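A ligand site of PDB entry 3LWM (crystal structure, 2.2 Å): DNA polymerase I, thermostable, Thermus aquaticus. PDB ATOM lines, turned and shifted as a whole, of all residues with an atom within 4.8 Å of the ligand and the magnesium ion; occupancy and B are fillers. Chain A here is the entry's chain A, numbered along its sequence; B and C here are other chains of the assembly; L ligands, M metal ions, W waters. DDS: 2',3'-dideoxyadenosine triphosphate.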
ATOM      1  N   ARG A 295      13.862 -15.017 -11.904  1.00  0.00           N
ATOM      2  CA  ARG A 295      13.299 -14.066 -10.939  1.00  0.00           C
ATOM      3  C   ARG A 295      13.787 -14.263  -9.491  1.00  0.00           C
ATOM      4  O   ARG A 295      13.618 -13.373  -8.659  1.00  0.00           O
ATOM      5  CB  ARG A 295      11.777 -14.068 -10.992  1.00  0.00           C
ATOM      6  CG  ARG A 295      11.207 -13.619 -12.338  1.00  0.00           C
ATOM      7  CD  ARG A 295       9.699 -13.833 -12.407  1.00  0.00           C
ATOM      8  NE  ARG A 295       9.182 -13.579 -13.751  1.00  0.00           N
ATOM      9  CZ  ARG A 295       7.912 -13.757 -14.118  1.00  0.00           C
ATOM     10  NH1 ARG A 295       7.021 -14.200 -13.235  1.00  0.00           N
ATOM     11  NH2 ARG A 295       7.533 -13.494 -15.368  1.00  0.00           N
ATOM     12  N   ASP A 318      16.094  -7.266 -25.763  1.00  0.00           N
ATOM     13  CA  ASP A 318      14.805  -7.246 -25.089  1.00  0.00           C
ATOM     14  C   ASP A 318      14.003  -5.989 -25.439  1.00  0.00           C
ATOM     15  O   ASP A 318      14.498  -4.866 -25.281  1.00  0.00           O
ATOM     16  CB  ASP A 318      15.055  -7.309 -23.572  1.00  0.00           C
ATOM     17  CG  ASP A 318      13.778  -7.315 -22.750  1.00  0.00           C
ATOM     18  OD1 ASP A 318      13.565  -8.296 -22.000  1.00  0.00           O
ATOM     19  OD2 ASP A 318      12.996  -6.348 -22.850  1.00  0.00           O
ATOM     20  N   SER A 320      11.701  -3.291 -24.493  1.00  0.00           N
ATOM     21  CA  SER A 320      11.240  -2.696 -23.247  1.00  0.00           C
ATOM     22  C   SER A 320       9.735  -2.420 -23.266  1.00  0.00           C
ATOM     23  O   SER A 320       9.251  -1.670 -24.115  1.00  0.00           O
ATOM     24  CB  SER A 320      11.994  -1.382 -22.965  1.00  0.00           C
ATOM     25  OG  SER A 320      13.404  -1.577 -22.984  1.00  0.00           O
ATOM     26  N   GLN A 321       9.006  -3.014 -22.327  1.00  0.00           N
ATOM     27  CA  GLN A 321       7.581  -2.748 -22.155  1.00  0.00           C
ATOM     28  C   GLN A 321       6.809  -2.782 -23.460  1.00  0.00           C
ATOM     29  O   GLN A 321       5.949  -1.939 -23.699  1.00  0.00           O
ATOM     30  CB  GLN A 321       7.365  -1.387 -21.496  1.00  0.00           C
ATOM     31  CG  GLN A 321       8.190  -1.129 -20.252  1.00  0.00           C
ATOM     32  CD  GLN A 321       9.328  -0.151 -20.483  1.00  0.00           C
ATOM     33  OE1 GLN A 321       9.322   0.595 -21.459  1.00  0.00           O
ATOM     34  NE2 GLN A 321      10.295  -0.149 -19.581  1.00  0.00           N
ATOM     35  N   GLU A 323       4.404  -4.633 -24.850  1.00  0.00           N
ATOM     36  CA  GLU A 323       2.952  -4.752 -24.818  1.00  0.00           C
ATOM     37  C   GLU A 323       2.276  -3.445 -24.397  1.00  0.00           C
ATOM     38  O   GLU A 323       1.215  -3.109 -24.915  1.00  0.00           O
ATOM     39  CB  GLU A 323       2.527  -5.952 -23.952  1.00  0.00           C
ATOM     40  CG  GLU A 323       2.947  -7.270 -24.584  1.00  0.00           C
ATOM     41  CD  GLU A 323       2.669  -8.472 -23.709  1.00  0.00           C
ATOM     42  OE1 GLU A 323       2.770  -9.619 -24.213  1.00  0.00           O
ATOM     43  OE2 GLU A 323       2.347  -8.283 -22.524  1.00  0.00           O
ATOM     44  N   LEU A 324       2.908  -2.703 -23.505  1.00  0.00           N
ATOM     45  CA  LEU A 324       2.400  -1.387 -23.109  1.00  0.00           C
ATOM     46  C   LEU A 324       2.516  -0.370 -24.248  1.00  0.00           C
ATOM     47  O   LEU A 324       1.619   0.445 -24.461  1.00  0.00           O
ATOM     48  CB  LEU A 324       3.130  -0.853 -21.883  1.00  0.00           C
ATOM     49  CG  LEU A 324       2.880  -1.580 -20.555  1.00  0.00           C
ATOM     50  CD1 LEU A 324       3.625  -0.891 -19.431  1.00  0.00           C
ATOM     51  CD2 LEU A 324       1.398  -1.641 -20.272  1.00  0.00           C
ATOM     52  N   HIS A 347       6.585   3.055 -16.092  1.00  0.00           N
ATOM     53  CA  HIS A 347       6.209   2.568 -14.771  1.00  0.00           C
ATOM     54  C   HIS A 347       6.475   3.643 -13.720  1.00  0.00           C
ATOM     55  O   HIS A 347       5.706   3.784 -12.759  1.00  0.00           O
ATOM     56  CB  HIS A 347       6.932   1.266 -14.433  1.00  0.00           C
ATOM     57  CG  HIS A 347       6.610   0.149 -15.381  1.00  0.00           C
ATOM     58  ND1 HIS A 347       5.321  -0.287 -15.611  1.00  0.00           N
ATOM     59  CD2 HIS A 347       7.404  -0.626 -16.153  1.00  0.00           C
ATOM     60  CE1 HIS A 347       5.339  -1.272 -16.488  1.00  0.00           C
ATOM     61  NE2 HIS A 347       6.595  -1.503 -16.823  1.00  0.00           N
ATOM     62  N   ARG A 367       7.611   1.658  -7.843  1.00  0.00           N
ATOM     63  CA  ARG A 367       7.597   1.415  -9.279  1.00  0.00           C
ATOM     64  C   ARG A 367       6.967   0.071  -9.617  1.00  0.00           C
ATOM     65  O   ARG A 367       6.164  -0.022 -10.552  1.00  0.00           O
ATOM     66  CB  ARG A 367       9.012   1.488  -9.874  1.00  0.00           C
ATOM     67  CG  ARG A 367       9.019   1.760 -11.379  1.00  0.00           C
ATOM     68  CD  ARG A 367      10.419   1.652 -11.973  1.00  0.00           C
ATOM     69  NE  ARG A 367      10.724   0.293 -12.397  1.00  0.00           N
ATOM     70  CZ  ARG A 367      10.754  -0.104 -13.672  1.00  0.00           C
ATOM     71  NH1 ARG A 367      10.513   0.758 -14.643  1.00  0.00           N
ATOM     72  NH2 ARG A 367      11.050  -1.366 -13.968  1.00  0.00           N
ATOM     73  N   ARG A 368       7.315  -0.961  -8.862  1.00  0.00           N
ATOM     74  CA  ARG A 368       6.713  -2.280  -9.056  1.00  0.00           C
ATOM     75  C   ARG A 368       5.206  -2.209  -8.793  1.00  0.00           C
ATOM     76  O   ARG A 368       4.423  -2.935  -9.410  1.00  0.00           O
ATOM     77  CB  ARG A 368       7.381  -3.334  -8.177  1.00  0.00           C
ATOM     78  CG  ARG A 368       6.559  -4.601  -7.939  1.00  0.00           C
ATOM     79  CD  ARG A 368       6.024  -5.222  -9.225  1.00  0.00           C
ATOM     80  NE  ARG A 368       7.018  -6.000  -9.965  1.00  0.00           N
ATOM     81  CZ  ARG A 368       6.720  -6.750 -11.022  1.00  0.00           C
ATOM     82  NH1 ARG A 368       5.472  -6.827 -11.466  1.00  0.00           N
ATOM     83  NH2 ARG A 368       7.682  -7.429 -11.643  1.00  0.00           N
ATOM     84  N   LYS A 371       3.901  -1.259 -12.051  1.00  0.00           N
ATOM     85  CA  LYS A 371       3.984  -2.387 -12.980  1.00  0.00           C
ATOM     86  C   LYS A 371       2.827  -3.340 -12.754  1.00  0.00           C
ATOM     87  O   LYS A 371       2.191  -3.819 -13.698  1.00  0.00           O
ATOM     88  CB  LYS A 371       5.305  -3.146 -12.813  1.00  0.00           C
ATOM     89  CG  LYS A 371       6.524  -2.460 -13.390  1.00  0.00           C
ATOM     90  CD  LYS A 371       7.756  -3.361 -13.305  1.00  0.00           C
ATOM     91  CE  LYS A 371       7.582  -4.641 -14.114  1.00  0.00           C
ATOM     92  NZ  LYS A 371       8.825  -5.465 -14.144  1.00  0.00           N
ATOM     93  N   PHE A 375       0.335  -4.357 -15.688  1.00  0.00           N
ATOM     94  CA  PHE A 375       0.099  -5.761 -15.996  1.00  0.00           C
ATOM     95  C   PHE A 375      -1.349  -6.133 -15.727  1.00  0.00           C
ATOM     96  O   PHE A 375      -1.986  -6.841 -16.503  1.00  0.00           O
ATOM     97  CB  PHE A 375       1.028  -6.665 -15.172  1.00  0.00           C
ATOM     98  CG  PHE A 375       2.485  -6.474 -15.461  1.00  0.00           C
ATOM     99  CD1 PHE A 375       2.908  -5.762 -16.567  1.00  0.00           C
ATOM    100  CD2 PHE A 375       3.450  -7.014 -14.618  1.00  0.00           C
ATOM    101  CE1 PHE A 375       4.251  -5.577 -16.836  1.00  0.00           C
ATOM    102  CE2 PHE A 375       4.797  -6.840 -14.874  1.00  0.00           C
ATOM    103  CZ  PHE A 375       5.196  -6.126 -15.987  1.00  0.00           C
ATOM    104  N   LEU A 378      -3.506  -5.022 -18.407  1.00  0.00           N
ATOM    105  CA  LEU A 378      -3.213  -5.882 -19.547  1.00  0.00           C
ATOM    106  C   LEU A 378      -4.038  -7.171 -19.503  1.00  0.00           C
ATOM    107  O   LEU A 378      -4.502  -7.647 -20.529  1.00  0.00           O
ATOM    108  CB  LEU A 378      -1.728  -6.230 -19.568  1.00  0.00           C
ATOM    109  CG  LEU A 378      -0.933  -6.022 -20.852  1.00  0.00           C
ATOM    110  CD1 LEU A 378      -0.810  -4.541 -21.164  1.00  0.00           C
ATOM    111  CD2 LEU A 378       0.442  -6.667 -20.740  1.00  0.00           C
ATOM    112  N   TYR A 379      -4.189  -7.738 -18.311  1.00  0.00           N
ATOM    113  CA  TYR A 379      -4.819  -9.048 -18.144  1.00  0.00           C
ATOM    114  C   TYR A 379      -6.245  -8.980 -17.610  1.00  0.00           C
ATOM    115  O   TYR A 379      -6.878 -10.023 -17.375  1.00  0.00           O
ATOM    116  CB  TYR A 379      -3.995  -9.918 -17.199  1.00  0.00           C
ATOM    117  CG  TYR A 379      -2.521 -10.011 -17.536  1.00  0.00           C
ATOM    118  CD1 TYR A 379      -2.088 -10.068 -18.844  1.00  0.00           C
ATOM    119  CD2 TYR A 379      -1.569 -10.077 -16.518  1.00  0.00           C
ATOM    120  CE1 TYR A 379      -0.735 -10.172 -19.141  1.00  0.00           C
ATOM    121  CE2 TYR A 379      -0.222 -10.184 -16.808  1.00  0.00           C
ATOM    122  CZ  TYR A 379       0.196 -10.225 -18.123  1.00  0.00           C
ATOM    123  OH  TYR A 379       1.536 -10.336 -18.406  1.00  0.00           O
ATOM    124  N   ASP A 493       9.349 -11.481 -25.944  1.00  0.00           N
ATOM    125  CA  ASP A 493       9.758 -10.100 -26.159  1.00  0.00           C
ATOM    126  C   ASP A 493      11.278  -9.974 -26.182  1.00  0.00           C
ATOM    127  O   ASP A 493      11.825  -8.885 -26.182  1.00  0.00           O
ATOM    128  CB  ASP A 493       9.172  -9.178 -25.083  1.00  0.00           C
ATOM    129  CG  ASP A 493       9.672  -9.507 -23.687  1.00  0.00           C
ATOM    130  OD1 ASP A 493      10.373 -10.524 -23.513  1.00  0.00           O
ATOM    131  OD2 ASP A 493       9.347  -8.747 -22.746  1.00  0.00           O
ATOM    132  P   2DA B  12      10.767 -13.596 -17.633  1.00  0.00           P
ATOM    133  OP1 2DA B  12      10.240 -12.891 -16.337  1.00  0.00           O
ATOM    134  OP2 2DA B  12      12.141 -13.124 -17.924  1.00  0.00           O
ATOM    135  O5' 2DA B  12       9.819 -13.202 -18.812  1.00  0.00           O
ATOM    136  C5' 2DA B  12      10.108 -13.607 -20.090  1.00  0.00           C
ATOM    137  C4' 2DA B  12       8.998 -13.393 -21.072  1.00  0.00           C
ATOM    138  O4' 2DA B  12       7.819 -14.313 -21.014  1.00  0.00           O
ATOM    139  C3' 2DA B  12       8.452 -11.980 -21.272  1.00  0.00           C
ATOM    140  C2' 2DA B  12       6.999 -12.158 -21.521  1.00  0.00           C
ATOM    141  C1' 2DA B  12       6.684 -13.423 -20.772  1.00  0.00           C
ATOM    142  N9  2DA B  12       5.930 -13.661 -19.582  1.00  0.00           N
ATOM    143  C8  2DA B  12       6.443 -13.598 -18.278  1.00  0.00           C
ATOM    144  N7  2DA B  12       5.447 -13.810 -17.431  1.00  0.00           N
ATOM    145  C5  2DA B  12       4.285 -13.984 -18.178  1.00  0.00           C
ATOM    146  C6  2DA B  12       2.963 -14.232 -17.785  1.00  0.00           C
ATOM    147  N6  2DA B  12       2.650 -14.336 -16.393  1.00  0.00           N
ATOM    148  N1  2DA B  12       1.984 -14.378 -18.754  1.00  0.00           N
ATOM    149  C2  2DA B  12       2.310 -14.270 -20.116  1.00  0.00           C
ATOM    150  N3  2DA B  12       3.601 -14.025 -20.496  1.00  0.00           N
ATOM    151  C4  2DA B  12       4.597 -13.885 -19.499  1.00  0.00           C
ATOM    152  O5'  DT C   1      -6.603 -13.745 -18.624  1.00  0.00           O
ATOM    153  C5'  DT C   1      -6.872 -12.761 -19.623  1.00  0.00           C
ATOM    154  C4'  DT C   1      -5.812 -12.833 -20.709  1.00  0.00           C
ATOM    155  O4'  DT C   1      -4.626 -12.129 -20.257  1.00  0.00           O
ATOM    156  C3'  DT C   1      -5.322 -14.239 -21.020  1.00  0.00           C
ATOM    157  O3'  DT C   1      -6.110 -14.822 -22.045  1.00  0.00           O
ATOM    158  C2'  DT C   1      -3.912 -13.988 -21.518  1.00  0.00           C
ATOM    159  C1'  DT C   1      -3.468 -12.801 -20.683  1.00  0.00           C
ATOM    160  N1   DT C   1      -2.662 -13.191 -19.506  1.00  0.00           N
ATOM    161  C2   DT C   1      -1.343 -13.545 -19.707  1.00  0.00           C
ATOM    162  O2   DT C   1      -0.821 -13.566 -20.806  1.00  0.00           O
ATOM    163  N3   DT C   1      -0.660 -13.877 -18.578  1.00  0.00           N
ATOM    164  C4   DT C   1      -1.150 -13.898 -17.290  1.00  0.00           C
ATOM    165  O4   DT C   1      -0.458 -14.215 -16.323  1.00  0.00           O
ATOM    166  C5   DT C   1      -2.539 -13.516 -17.145  1.00  0.00           C
ATOM    167  C7   DT C   1      -3.170 -13.504 -15.786  1.00  0.00           C
ATOM    168  C6   DT C   1      -3.223 -13.186 -18.246  1.00  0.00           C
HETATM  169  N1  DDS L   1       3.485 -11.435 -13.539  1.00  0.00           N
HETATM  170  C2  DDS L   1       2.699 -11.314 -14.635  1.00  0.00           C
HETATM  171  N3  DDS L   1       3.160 -10.896 -15.831  1.00  0.00           N
HETATM  172  C4  DDS L   1       4.468 -10.570 -15.993  1.00  0.00           C
HETATM  173  C5  DDS L   1       5.379 -10.661 -14.850  1.00  0.00           C
HETATM  174  C6  DDS L   1       4.799 -11.136 -13.560  1.00  0.00           C
HETATM  175  N6  DDS L   1       5.569 -11.255 -12.449  1.00  0.00           N
HETATM  176  N7  DDS L   1       6.599 -10.280 -15.278  1.00  0.00           N
HETATM  177  C8  DDS L   1       6.474  -9.956 -16.590  1.00  0.00           C
HETATM  178  N9  DDS L   1       5.204 -10.109 -17.019  1.00  0.00           N
HETATM  179  PA  DDS L   1       9.107  -7.071 -17.896  1.00  0.00           P
HETATM  180  PB  DDS L   1       8.528  -4.358 -18.325  1.00  0.00           P
HETATM  181  PG  DDS L   1      10.583  -3.273 -16.719  1.00  0.00           P
HETATM  182  C1' DDS L   1       4.696  -9.872 -18.393  1.00  0.00           C
HETATM  183  O1A DDS L   1       8.930  -8.070 -16.778  1.00  0.00           O
HETATM  184  O1B DDS L   1       9.619  -4.539 -19.376  1.00  0.00           O
HETATM  185  O1G DDS L   1      10.994  -1.851 -17.045  1.00  0.00           O
HETATM  186  C2' DDS L   1       4.320  -8.407 -18.580  1.00  0.00           C
HETATM  187  O2A DDS L   1      10.495  -6.734 -18.374  1.00  0.00           O
HETATM  188  O2B DDS L   1       7.142  -3.939 -18.751  1.00  0.00           O
HETATM  189  O2G DDS L   1      10.516  -3.548 -15.244  1.00  0.00           O
HETATM  190  C3' DDS L   1       5.540  -7.771 -19.224  1.00  0.00           C
HETATM  191  O3A DDS L   1       8.406  -5.691 -17.435  1.00  0.00           O
HETATM  192  O3B DDS L   1       9.048  -3.307 -17.215  1.00  0.00           O
HETATM  193  O3G DDS L   1      11.264  -4.358 -17.514  1.00  0.00           O
HETATM  194  C4' DDS L   1       6.349  -8.925 -19.781  1.00  0.00           C
HETATM  195  O4' DDS L   1       5.750 -10.142 -19.316  1.00  0.00           O
HETATM  196  C5' DDS L   1       7.774  -8.875 -19.250  1.00  0.00           C
HETATM  197  O5' DDS L   1       8.216  -7.531 -19.156  1.00  0.00           O
HETATM  198 MG    MG M   1      11.807  -5.495 -19.464  1.00  0.00          MG
HETATM  199  O   HOH W   1      12.262  -3.337 -20.070  1.00  0.00           O
HETATM  200  O   HOH W   2      11.124  -8.836 -20.532  1.00  0.00           O
HETATM  201  O   HOH W   3       4.095 -14.485 -13.956  1.00  0.00           O
HETATM  202  O   HOH W   4      10.868  -5.796 -21.330  1.00  0.00           O
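Phe 375 touches the ligand.
Asp 493 touches the ligand (OD2 to C5', 3.8 Å).
2DA 12 of chain B touches the ligand.
Hydrophobic or aromatic side chains within 4 Å of the ligand: His 347, Phe 375 and Tyr 379.
Nine residues have an atom within 4 Å of the ligand: Arg 295, Gln 321, His 347, Arg 367, Lys 371, Phe 375, Tyr 379, Asp 493 and 2DA 12 of chain B.
The magnesium ion is bound by O2A of the ligand (2.1 Å), water W4 (2.1 Å), water W1 (2.3 Å), O3G of the ligand (2.3 Å) and O1B of the ligand (2.4 Å).
The magnesium ion has five donor atoms within binding distance.
O2G of the ligand is in salt-bridge range of NZ of Lys 371, at 2.8 Å.
The guanidinium group (NH2) of Arg 367 lies within salt-bridge range of an oxygen (O2G) of the ligand, 2.6 Å away.
O1G of the ligand is in hydrogen-bond range of NE2 of Gln 321 (3.1 Å).
A ring nitrogen (NE2) of His 347 lies within hydrogen-bond range of an oxygen (O3B) of the ligand, at 3.1 Å.
The backbone NH of Gln 321 lies close to an oxygen (O1B) of the ligand (3.4 Å).
The guanidinium group of Arg 295 is in hydrogen-bond range of a nitrogen (N7) of the ligand.
A nitrogen (N3) of the ligand is in hydrogen-bond range of the side-chain hydroxyl of Tyr 379, 3.1 Å away.
Water W4 bridges OD2 of Asp 318 (2.7 Å) and N of Gln 321 (3.5 Å).
Water W3 lies within hydrogen-bond range of N6 of 2DA 12 of chain B, NH1 of Arg 295 and N1 of the ligand.
The guanidinium group (NE) of Arg 295 is in salt-bridge range of OP1 of 2DA 12 of chain B, 2.9 Å away.
N1 of 2DA 12 of chain B lies close to N3 of DT 1 of chain C, 2.7 Å away.
Merely in contact with the magnesium ion: Asp 318.
The nearest printed residue that does not touch the magnesium ion is Gln 321 (4.7 Å).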
